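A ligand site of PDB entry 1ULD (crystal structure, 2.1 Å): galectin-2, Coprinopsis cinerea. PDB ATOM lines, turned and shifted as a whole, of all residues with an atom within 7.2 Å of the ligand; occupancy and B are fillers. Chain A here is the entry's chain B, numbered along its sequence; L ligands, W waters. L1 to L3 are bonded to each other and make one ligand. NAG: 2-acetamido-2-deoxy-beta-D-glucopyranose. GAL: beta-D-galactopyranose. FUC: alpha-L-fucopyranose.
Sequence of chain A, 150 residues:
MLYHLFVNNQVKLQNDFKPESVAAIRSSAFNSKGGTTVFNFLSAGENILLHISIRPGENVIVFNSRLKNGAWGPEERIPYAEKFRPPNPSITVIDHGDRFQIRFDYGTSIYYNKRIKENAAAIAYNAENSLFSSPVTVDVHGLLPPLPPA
A ring nitrogen (NE2) of His 51 is in hydrogen-bond range of an oxygen (O4) of GAL L2, 2.7 Å away.
OE2 of Glu 75 lies within hydrogen-bond range of O3 of NAG L1.
An oxygen (O3) of NAG L1 sits at hydrogen-bond distance from the guanidinium group (NH1) of Arg 55.
NH2 of Arg 77 lies within hydrogen-bond range of O3 of NAG L1 (3.1 Å).
O6 of GAL L2 sits at hydrogen-bond distance from ND2 of Asn 64 (2.9 Å).
The backbone carbonyl oxygen of Val 60 sits at hydrogen-bond distance from the backbone NH of Arg 55, 2.9 Å away.
The side-chain amide nitrogen (ND2) of Asn 64 is in hydrogen-bond range of the backbone carbonyl oxygen (O) of Gly 73.
The backbone carbonyl oxygen (O) of Asn 64 sits at hydrogen-bond distance from the backbone NH (N) of His 51 (2.8 Å).
The side-chain carboxylate (OE1) of Glu 58 is in salt-bridge range of the guanidinium group (NH1) of Arg 55, 3.0 Å away.
The backbone carbonyl oxygen (O) of Ser 53 sits at hydrogen-bond distance from the backbone NH (N) of Val 62 (2.8 Å).
OE1 of Glu 75 is in salt-bridge range of NE of Arg 77 (2.9 Å).
The side-chain hydroxyl (OG) of Ser 53 sits at hydrogen-bond distance from the guanidinium group (NE) of Arg 55, 3.0 Å away.
The guanidinium group (NH1) of Arg 77 is in salt-bridge range of the side-chain carboxylate (OE2) of Glu 58.
CB of Ser 53 touches O4 of GAL L2, 3.6 Å away.
Val 62 touches the ligand.
NE1 of Trp 72 touches C5 of GAL L2 (3.6 Å).
Hydrophobic or aromatic side chains that line the ligand: His 51, Val 62 and Trp 72.
Water W5 bridges an oxygen (O7) of NAG L1 (2.6 Å) and the side-chain carboxylate (OE1) of Glu 75 (2.9 Å).
Water W2 lies within hydrogen-bond range of a nitrogen (N2) of NAG L1, the side-chain carboxylate (OE2) of Glu 58 and the guanidinium group (NH2) of Arg 77.
Water W7 lies within hydrogen-bond range of the side-chain hydroxyl (OG) of Ser 53 and an oxygen (O4) of GAL L2.
Water W6 lies within hydrogen-bond range of O6 of NAG L1 (3.3 Å) and OE2 of Glu 75 (3.4 Å).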
ATOM      1  N   THR A  36      -6.153 -10.350  33.478  1.00  0.00           N
ATOM      2  CA  THR A  36      -5.144 -11.200  32.881  1.00  0.00           C
ATOM      3  C   THR A  36      -4.097 -10.360  32.161  1.00  0.00           C
ATOM      4  O   THR A  36      -4.417  -9.487  31.351  1.00  0.00           O
ATOM      5  CB  THR A  36      -5.823 -12.213  31.926  1.00  0.00           C
ATOM      6  OG1 THR A  36      -6.641 -13.103  32.710  1.00  0.00           O
ATOM      7  CG2 THR A  36      -4.794 -13.040  31.158  1.00  0.00           C
ATOM      8  N   VAL A  38      -0.318 -10.629  30.068  1.00  0.00           N
ATOM      9  CA  VAL A  38       0.566 -11.540  29.346  1.00  0.00           C
ATOM     10  C   VAL A  38       1.885 -10.936  28.869  1.00  0.00           C
ATOM     11  O   VAL A  38       1.950  -9.765  28.476  1.00  0.00           O
ATOM     12  CB  VAL A  38      -0.162 -12.106  28.068  1.00  0.00           C
ATOM     13  CG1 VAL A  38       0.829 -12.846  27.169  1.00  0.00           C
ATOM     14  CG2 VAL A  38      -1.310 -13.036  28.482  1.00  0.00           C
ATOM     15  N   HIS A  51       5.298 -18.065  26.536  1.00  0.00           N
ATOM     16  CA  HIS A  51       4.066 -17.319  26.791  1.00  0.00           C
ATOM     17  C   HIS A  51       3.826 -17.391  28.291  1.00  0.00           C
ATOM     18  O   HIS A  51       3.855 -18.470  28.879  1.00  0.00           O
ATOM     19  CB  HIS A  51       2.893 -17.982  26.053  1.00  0.00           C
ATOM     20  CG  HIS A  51       1.549 -17.403  26.400  1.00  0.00           C
ATOM     21  ND1 HIS A  51       1.136 -16.165  25.978  1.00  0.00           N
ATOM     22  CD2 HIS A  51       0.517 -17.930  27.097  1.00  0.00           C
ATOM     23  CE1 HIS A  51      -0.103 -15.951  26.383  1.00  0.00           C
ATOM     24  NE2 HIS A  51      -0.506 -17.010  27.070  1.00  0.00           N
ATOM     25  N   ILE A  52       3.625 -16.227  28.898  1.00  0.00           N
ATOM     26  CA  ILE A  52       3.367 -16.140  30.336  1.00  0.00           C
ATOM     27  C   ILE A  52       2.045 -15.408  30.515  1.00  0.00           C
ATOM     28  O   ILE A  52       1.957 -14.196  30.294  1.00  0.00           O
ATOM     29  CB  ILE A  52       4.490 -15.344  31.067  1.00  0.00           C
ATOM     30  CG1 ILE A  52       5.862 -15.982  30.794  1.00  0.00           C
ATOM     31  CG2 ILE A  52       4.218 -15.345  32.570  1.00  0.00           C
ATOM     32  CD1 ILE A  52       7.051 -15.194  31.366  1.00  0.00           C
ATOM     33  N   SER A  53       1.017 -16.155  30.910  1.00  0.00           N
ATOM     34  CA  SER A  53      -0.307 -15.587  31.117  1.00  0.00           C
ATOM     35  C   SER A  53      -0.633 -15.585  32.611  1.00  0.00           C
ATOM     36  O   SER A  53      -0.882 -16.637  33.191  1.00  0.00           O
ATOM     37  CB  SER A  53      -1.359 -16.399  30.349  1.00  0.00           C
ATOM     38  OG  SER A  53      -2.670 -15.879  30.549  1.00  0.00           O
ATOM     39  N   ILE A  54      -0.616 -14.393  33.203  1.00  0.00           N
ATOM     40  CA  ILE A  54      -0.915 -14.212  34.623  1.00  0.00           C
ATOM     41  C   ILE A  54      -2.405 -13.912  34.741  1.00  0.00           C
ATOM     42  O   ILE A  54      -2.872 -12.868  34.273  1.00  0.00           O
ATOM     43  CB  ILE A  54      -0.095 -13.039  35.198  1.00  0.00           C
ATOM     44  CG1 ILE A  54       1.394 -13.287  34.963  1.00  0.00           C
ATOM     45  CG2 ILE A  54      -0.392 -12.869  36.692  1.00  0.00           C
ATOM     46  CD1 ILE A  54       2.245 -12.025  35.021  1.00  0.00           C
ATOM     47  N   ARG A  55      -3.143 -14.828  35.366  1.00  0.00           N
ATOM     48  CA  ARG A  55      -4.593 -14.680  35.488  1.00  0.00           C
ATOM     49  C   ARG A  55      -5.091 -14.552  36.927  1.00  0.00           C
ATOM     50  O   ARG A  55      -5.215 -15.550  37.644  1.00  0.00           O
ATOM     51  CB  ARG A  55      -5.275 -15.872  34.824  1.00  0.00           C
ATOM     52  CG  ARG A  55      -4.730 -16.187  33.435  1.00  0.00           C
ATOM     53  CD  ARG A  55      -5.382 -17.424  32.844  1.00  0.00           C
ATOM     54  NE  ARG A  55      -4.780 -17.810  31.573  1.00  0.00           N
ATOM     55  CZ  ARG A  55      -5.135 -18.896  30.875  1.00  0.00           C
ATOM     56  NH1 ARG A  55      -6.094 -19.696  31.334  1.00  0.00           N
ATOM     57  NH2 ARG A  55      -4.536 -19.180  29.728  1.00  0.00           N
ATOM     58  N   GLU A  58      -8.727 -16.479  37.543  1.00  0.00           N
ATOM     59  CA  GLU A  58      -8.583 -17.928  37.615  1.00  0.00           C
ATOM     60  C   GLU A  58      -7.558 -18.308  38.672  1.00  0.00           C
ATOM     61  O   GLU A  58      -7.484 -19.470  39.100  1.00  0.00           O
ATOM     62  CB  GLU A  58      -8.139 -18.453  36.250  1.00  0.00           C
ATOM     63  CG  GLU A  58      -8.456 -19.905  35.995  1.00  0.00           C
ATOM     64  CD  GLU A  58      -7.972 -20.351  34.640  1.00  0.00           C
ATOM     65  OE1 GLU A  58      -7.919 -19.502  33.717  1.00  0.00           O
ATOM     66  OE2 GLU A  58      -7.653 -21.550  34.490  1.00  0.00           O
ATOM     67  N   VAL A  60      -4.184 -18.372  38.450  1.00  0.00           N
ATOM     68  CA  VAL A  60      -3.162 -19.264  37.927  1.00  0.00           C
ATOM     69  C   VAL A  60      -2.249 -18.480  37.006  1.00  0.00           C
ATOM     70  O   VAL A  60      -2.547 -17.351  36.613  1.00  0.00           O
ATOM     71  CB  VAL A  60      -3.749 -20.435  37.079  1.00  0.00           C
ATOM     72  CG1 VAL A  60      -4.743 -21.244  37.896  1.00  0.00           C
ATOM     73  CG2 VAL A  60      -4.389 -19.883  35.811  1.00  0.00           C
ATOM     74  N   VAL A  62      -0.246 -19.356  33.514  1.00  0.00           N
ATOM     75  CA  VAL A  62      -0.078 -20.364  32.469  1.00  0.00           C
ATOM     76  C   VAL A  62       1.119 -20.075  31.595  1.00  0.00           C
ATOM     77  O   VAL A  62       1.291 -18.959  31.100  1.00  0.00           O
ATOM     78  CB  VAL A  62      -1.341 -20.440  31.573  1.00  0.00           C
ATOM     79  CG1 VAL A  62      -1.201 -21.598  30.585  1.00  0.00           C
ATOM     80  CG2 VAL A  62      -2.574 -20.607  32.427  1.00  0.00           C
ATOM     81  N   PHE A  63       1.965 -21.086  31.424  1.00  0.00           N
ATOM     82  CA  PHE A  63       3.145 -20.979  30.584  1.00  0.00           C
ATOM     83  C   PHE A  63       2.896 -21.905  29.377  1.00  0.00           C
ATOM     84  O   PHE A  63       2.426 -23.036  29.540  1.00  0.00           O
ATOM     85  CB  PHE A  63       4.395 -21.444  31.331  1.00  0.00           C
ATOM     86  CG  PHE A  63       4.691 -20.648  32.577  1.00  0.00           C
ATOM     87  CD1 PHE A  63       4.124 -21.002  33.799  1.00  0.00           C
ATOM     88  CD2 PHE A  63       5.550 -19.553  32.527  1.00  0.00           C
ATOM     89  CE1 PHE A  63       4.402 -20.272  34.963  1.00  0.00           C
ATOM     90  CE2 PHE A  63       5.843 -18.805  33.685  1.00  0.00           C
ATOM     91  CZ  PHE A  63       5.266 -19.178  34.903  1.00  0.00           C
ATOM     92  N   ASN A  64       3.220 -21.421  28.186  1.00  0.00           N
ATOM     93  CA  ASN A  64       3.015 -22.218  26.984  1.00  0.00           C
ATOM     94  C   ASN A  64       3.897 -21.676  25.874  1.00  0.00           C
ATOM     95  O   ASN A  64       4.611 -20.690  26.062  1.00  0.00           O
ATOM     96  CB  ASN A  64       1.547 -22.148  26.541  1.00  0.00           C
ATOM     97  CG  ASN A  64       1.064 -23.444  25.897  1.00  0.00           C
ATOM     98  OD1 ASN A  64       1.847 -24.231  25.352  1.00  0.00           O
ATOM     99  ND2 ASN A  64      -0.259 -23.659  25.936  1.00  0.00           N
ATOM    100  N   SER A  65       3.833 -22.318  24.717  1.00  0.00           N
ATOM    101  CA  SER A  65       4.588 -21.943  23.524  1.00  0.00           C
ATOM    102  C   SER A  65       3.669 -22.220  22.329  1.00  0.00           C
ATOM    103  O   SER A  65       2.692 -22.963  22.458  1.00  0.00           O
ATOM    104  CB  SER A  65       5.852 -22.798  23.390  1.00  0.00           C
ATOM    105  OG  SER A  65       6.722 -22.646  24.496  1.00  0.00           O
ATOM    106  N   ARG A  66       3.981 -21.631  21.183  1.00  0.00           N
ATOM    107  CA  ARG A  66       3.176 -21.844  19.986  1.00  0.00           C
ATOM    108  C   ARG A  66       3.839 -21.250  18.757  1.00  0.00           C
ATOM    109  O   ARG A  66       4.483 -20.198  18.832  1.00  0.00           O
ATOM    110  CB  ARG A  66       1.776 -21.240  20.176  1.00  0.00           C
ATOM    111  CG  ARG A  66       1.419 -20.176  19.167  1.00  0.00           C
ATOM    112  CD  ARG A  66       0.235 -19.329  19.587  1.00  0.00           C
ATOM    113  NE  ARG A  66       0.126 -18.179  18.690  1.00  0.00           N
ATOM    114  CZ  ARG A  66      -0.595 -17.095  18.936  1.00  0.00           C
ATOM    115  NH1 ARG A  66      -1.290 -16.987  20.069  1.00  0.00           N
ATOM    116  NH2 ARG A  66      -0.603 -16.094  18.056  1.00  0.00           N
ATOM    117  N   TRP A  72      -1.739 -23.614  20.484  1.00  0.00           N
ATOM    118  CA  TRP A  72      -1.013 -23.662  21.750  1.00  0.00           C
ATOM    119  C   TRP A  72      -0.682 -25.105  22.088  1.00  0.00           C
ATOM    120  O   TRP A  72      -1.445 -26.015  21.785  1.00  0.00           O
ATOM    121  CB  TRP A  72      -1.851 -23.071  22.876  1.00  0.00           C
ATOM    122  CG  TRP A  72      -2.050 -21.598  22.790  1.00  0.00           C
ATOM    123  CD1 TRP A  72      -3.219 -20.939  22.472  1.00  0.00           C
ATOM    124  CD2 TRP A  72      -1.078 -20.581  23.046  1.00  0.00           C
ATOM    125  NE1 TRP A  72      -3.021 -19.581  22.529  1.00  0.00           N
ATOM    126  CE2 TRP A  72      -1.712 -19.335  22.879  1.00  0.00           C
ATOM    127  CE3 TRP A  72       0.279 -20.618  23.405  1.00  0.00           C
ATOM    128  CZ2 TRP A  72      -1.041 -18.118  23.048  1.00  0.00           C
ATOM    129  CZ3 TRP A  72       0.942 -19.413  23.583  1.00  0.00           C
ATOM    130  CH2 TRP A  72       0.282 -18.178  23.401  1.00  0.00           C
ATOM    131  N   GLY A  73       0.462 -25.315  22.737  1.00  0.00           N
ATOM    132  CA  GLY A  73       0.851 -26.658  23.129  1.00  0.00           C
ATOM    133  C   GLY A  73       0.233 -26.980  24.467  1.00  0.00           C
ATOM    134  O   GLY A  73      -0.704 -26.306  24.891  1.00  0.00           O
ATOM    135  N   PRO A  74       0.711 -28.029  25.156  1.00  0.00           N
ATOM    136  CA  PRO A  74       0.129 -28.361  26.460  1.00  0.00           C
ATOM    137  C   PRO A  74       0.494 -27.247  27.442  1.00  0.00           C
ATOM    138  O   PRO A  74       1.594 -26.699  27.387  1.00  0.00           O
ATOM    139  CB  PRO A  74       0.808 -29.693  26.800  1.00  0.00           C
ATOM    140  CG  PRO A  74       2.168 -29.539  26.167  1.00  0.00           C
ATOM    141  CD  PRO A  74       1.830 -28.930  24.825  1.00  0.00           C
ATOM    142  N   GLU A  75      -0.440 -26.909  28.330  1.00  0.00           N
ATOM    143  CA  GLU A  75      -0.187 -25.846  29.290  1.00  0.00           C
ATOM    144  C   GLU A  75       0.601 -26.322  30.492  1.00  0.00           C
ATOM    145  O   GLU A  75       0.500 -27.472  30.895  1.00  0.00           O
ATOM    146  CB  GLU A  75      -1.502 -25.251  29.782  1.00  0.00           C
ATOM    147  CG  GLU A  75      -2.416 -24.727  28.708  1.00  0.00           C
ATOM    148  CD  GLU A  75      -3.558 -23.917  29.278  1.00  0.00           C
ATOM    149  OE1 GLU A  75      -4.081 -24.303  30.343  1.00  0.00           O
ATOM    150  OE2 GLU A  75      -3.938 -22.898  28.666  1.00  0.00           O
ATOM    151  N   GLU A  76       1.416 -25.425  31.030  1.00  0.00           N
ATOM    152  CA  GLU A  76       2.172 -25.714  32.239  1.00  0.00           C
ATOM    153  C   GLU A  76       1.712 -24.609  33.184  1.00  0.00           C
ATOM    154  O   GLU A  76       2.100 -23.452  33.038  1.00  0.00           O
ATOM    155  CB  GLU A  76       3.677 -25.642  31.969  1.00  0.00           C
ATOM    156  CG  GLU A  76       4.208 -26.893  31.247  1.00  0.00           C
ATOM    157  CD  GLU A  76       5.713 -26.885  31.000  1.00  0.00           C
ATOM    158  OE1 GLU A  76       6.480 -26.677  31.963  1.00  0.00           O
ATOM    159  OE2 GLU A  76       6.117 -27.109  29.842  1.00  0.00           O
ATOM    160  N   ARG A  77       0.852 -24.969  34.133  1.00  0.00           N
ATOM    161  CA  ARG A  77       0.335 -23.962  35.049  1.00  0.00           C
ATOM    162  C   ARG A  77       0.733 -24.136  36.505  1.00  0.00           C
ATOM    163  O   ARG A  77       1.139 -25.206  36.942  1.00  0.00           O
ATOM    164  CB  ARG A  77      -1.195 -23.848  34.928  1.00  0.00           C
ATOM    165  CG  ARG A  77      -1.910 -24.980  34.173  1.00  0.00           C
ATOM    166  CD  ARG A  77      -3.437 -24.860  34.301  1.00  0.00           C
ATOM    167  NE  ARG A  77      -4.075 -24.066  33.251  1.00  0.00           N
ATOM    168  CZ  ARG A  77      -5.210 -23.373  33.421  1.00  0.00           C
ATOM    169  NH1 ARG A  77      -5.813 -23.375  34.605  1.00  0.00           N
ATOM    170  NH2 ARG A  77      -5.746 -22.698  32.419  1.00  0.00           N
HETATM  171  C1  NAG L   1      -9.037 -23.576  27.853  1.00  0.00           C
HETATM  172  C2  NAG L   1      -7.782 -23.465  28.703  1.00  0.00           C
HETATM  173  C3  NAG L   1      -7.284 -22.029  28.656  1.00  0.00           C
HETATM  174  C4  NAG L   1      -7.047 -21.607  27.199  1.00  0.00           C
HETATM  175  C5  NAG L   1      -8.294 -21.879  26.347  1.00  0.00           C
HETATM  176  C6  NAG L   1      -8.072 -21.643  24.866  1.00  0.00           C
HETATM  177  C7  NAG L   1      -7.763 -25.062  30.487  1.00  0.00           C
HETATM  178  C8  NAG L   1      -8.360 -25.505  31.813  1.00  0.00           C
HETATM  179  N2  NAG L   1      -8.073 -23.837  30.071  1.00  0.00           N
HETATM  180  O1  NAG L   1      -9.507 -24.873  27.891  1.00  0.00           O
HETATM  181  O3  NAG L   1      -6.080 -21.907  29.390  1.00  0.00           O
HETATM  182  O4  NAG L   1      -6.759 -20.199  27.184  1.00  0.00           O
HETATM  183  O5  NAG L   1      -8.726 -23.250  26.493  1.00  0.00           O
HETATM  184  O6  NAG L   1      -6.896 -22.294  24.418  1.00  0.00           O
HETATM  185  O7  NAG L   1      -7.039 -25.821  29.843  1.00  0.00           O
HETATM  186  C1  GAL L   2      -5.751 -19.754  26.356  1.00  0.00           C
HETATM  187  C2  GAL L   2      -5.828 -18.233  26.277  1.00  0.00           C
HETATM  188  C3  GAL L   2      -4.621 -17.650  25.547  1.00  0.00           C
HETATM  189  C4  GAL L   2      -3.308 -18.217  26.102  1.00  0.00           C
HETATM  190  C5  GAL L   2      -3.380 -19.748  26.104  1.00  0.00           C
HETATM  191  C6  GAL L   2      -2.137 -20.401  26.668  1.00  0.00           C
HETATM  192  O2  GAL L   2      -7.038 -17.876  25.573  1.00  0.00           O
HETATM  193  O3  GAL L   2      -4.629 -16.231  25.705  1.00  0.00           O
HETATM  194  O4  GAL L   2      -3.096 -17.739  27.436  1.00  0.00           O
HETATM  195  O5  GAL L   2      -4.498 -20.179  26.909  1.00  0.00           O
HETATM  196  O6  GAL L   2      -2.326 -21.805  26.849  1.00  0.00           O
HETATM  197  C1  FUC L   3      -7.705 -16.715  25.980  1.00  0.00           C
HETATM  198  C2  FUC L   3      -8.879 -16.436  25.039  1.00  0.00           C
HETATM  199  C3  FUC L   3      -9.995 -17.471  25.243  1.00  0.00           C
HETATM  200  C4  FUC L   3     -10.392 -17.556  26.721  1.00  0.00           C
HETATM  201  C5  FUC L   3      -9.146 -17.811  27.582  1.00  0.00           C
HETATM  202  C6  FUC L   3      -9.442 -17.807  29.071  1.00  0.00           C
HETATM  203  O2  FUC L   3      -8.432 -16.484  23.687  1.00  0.00           O
HETATM  204  O3  FUC L   3     -11.127 -17.089  24.475  1.00  0.00           O
HETATM  205  O4  FUC L   3     -11.002 -16.342  27.118  1.00  0.00           O
HETATM  206  O5  FUC L   3      -8.156 -16.796  27.330  1.00  0.00           O
HETATM  207  O   HOH W   1      -6.852 -18.711  22.591  1.00  0.00           O
HETATM  208  O   HOH W   2      -8.827 -22.052  31.936  1.00  0.00           O
HETATM  209  O   HOH W   3      -3.588 -15.111  23.595  1.00  0.00           O
HETATM  210  O   HOH W   4      -6.648 -15.769  29.367  1.00  0.00           O
HETATM  211  O   HOH W   5      -4.774 -27.120  30.160  1.00  0.00           O
HETATM  212  O   HOH W   6      -4.673 -24.342  25.694  1.00  0.00           O
HETATM  213  O   HOH W   7      -4.006 -15.292  28.415  1.00  0.00           O
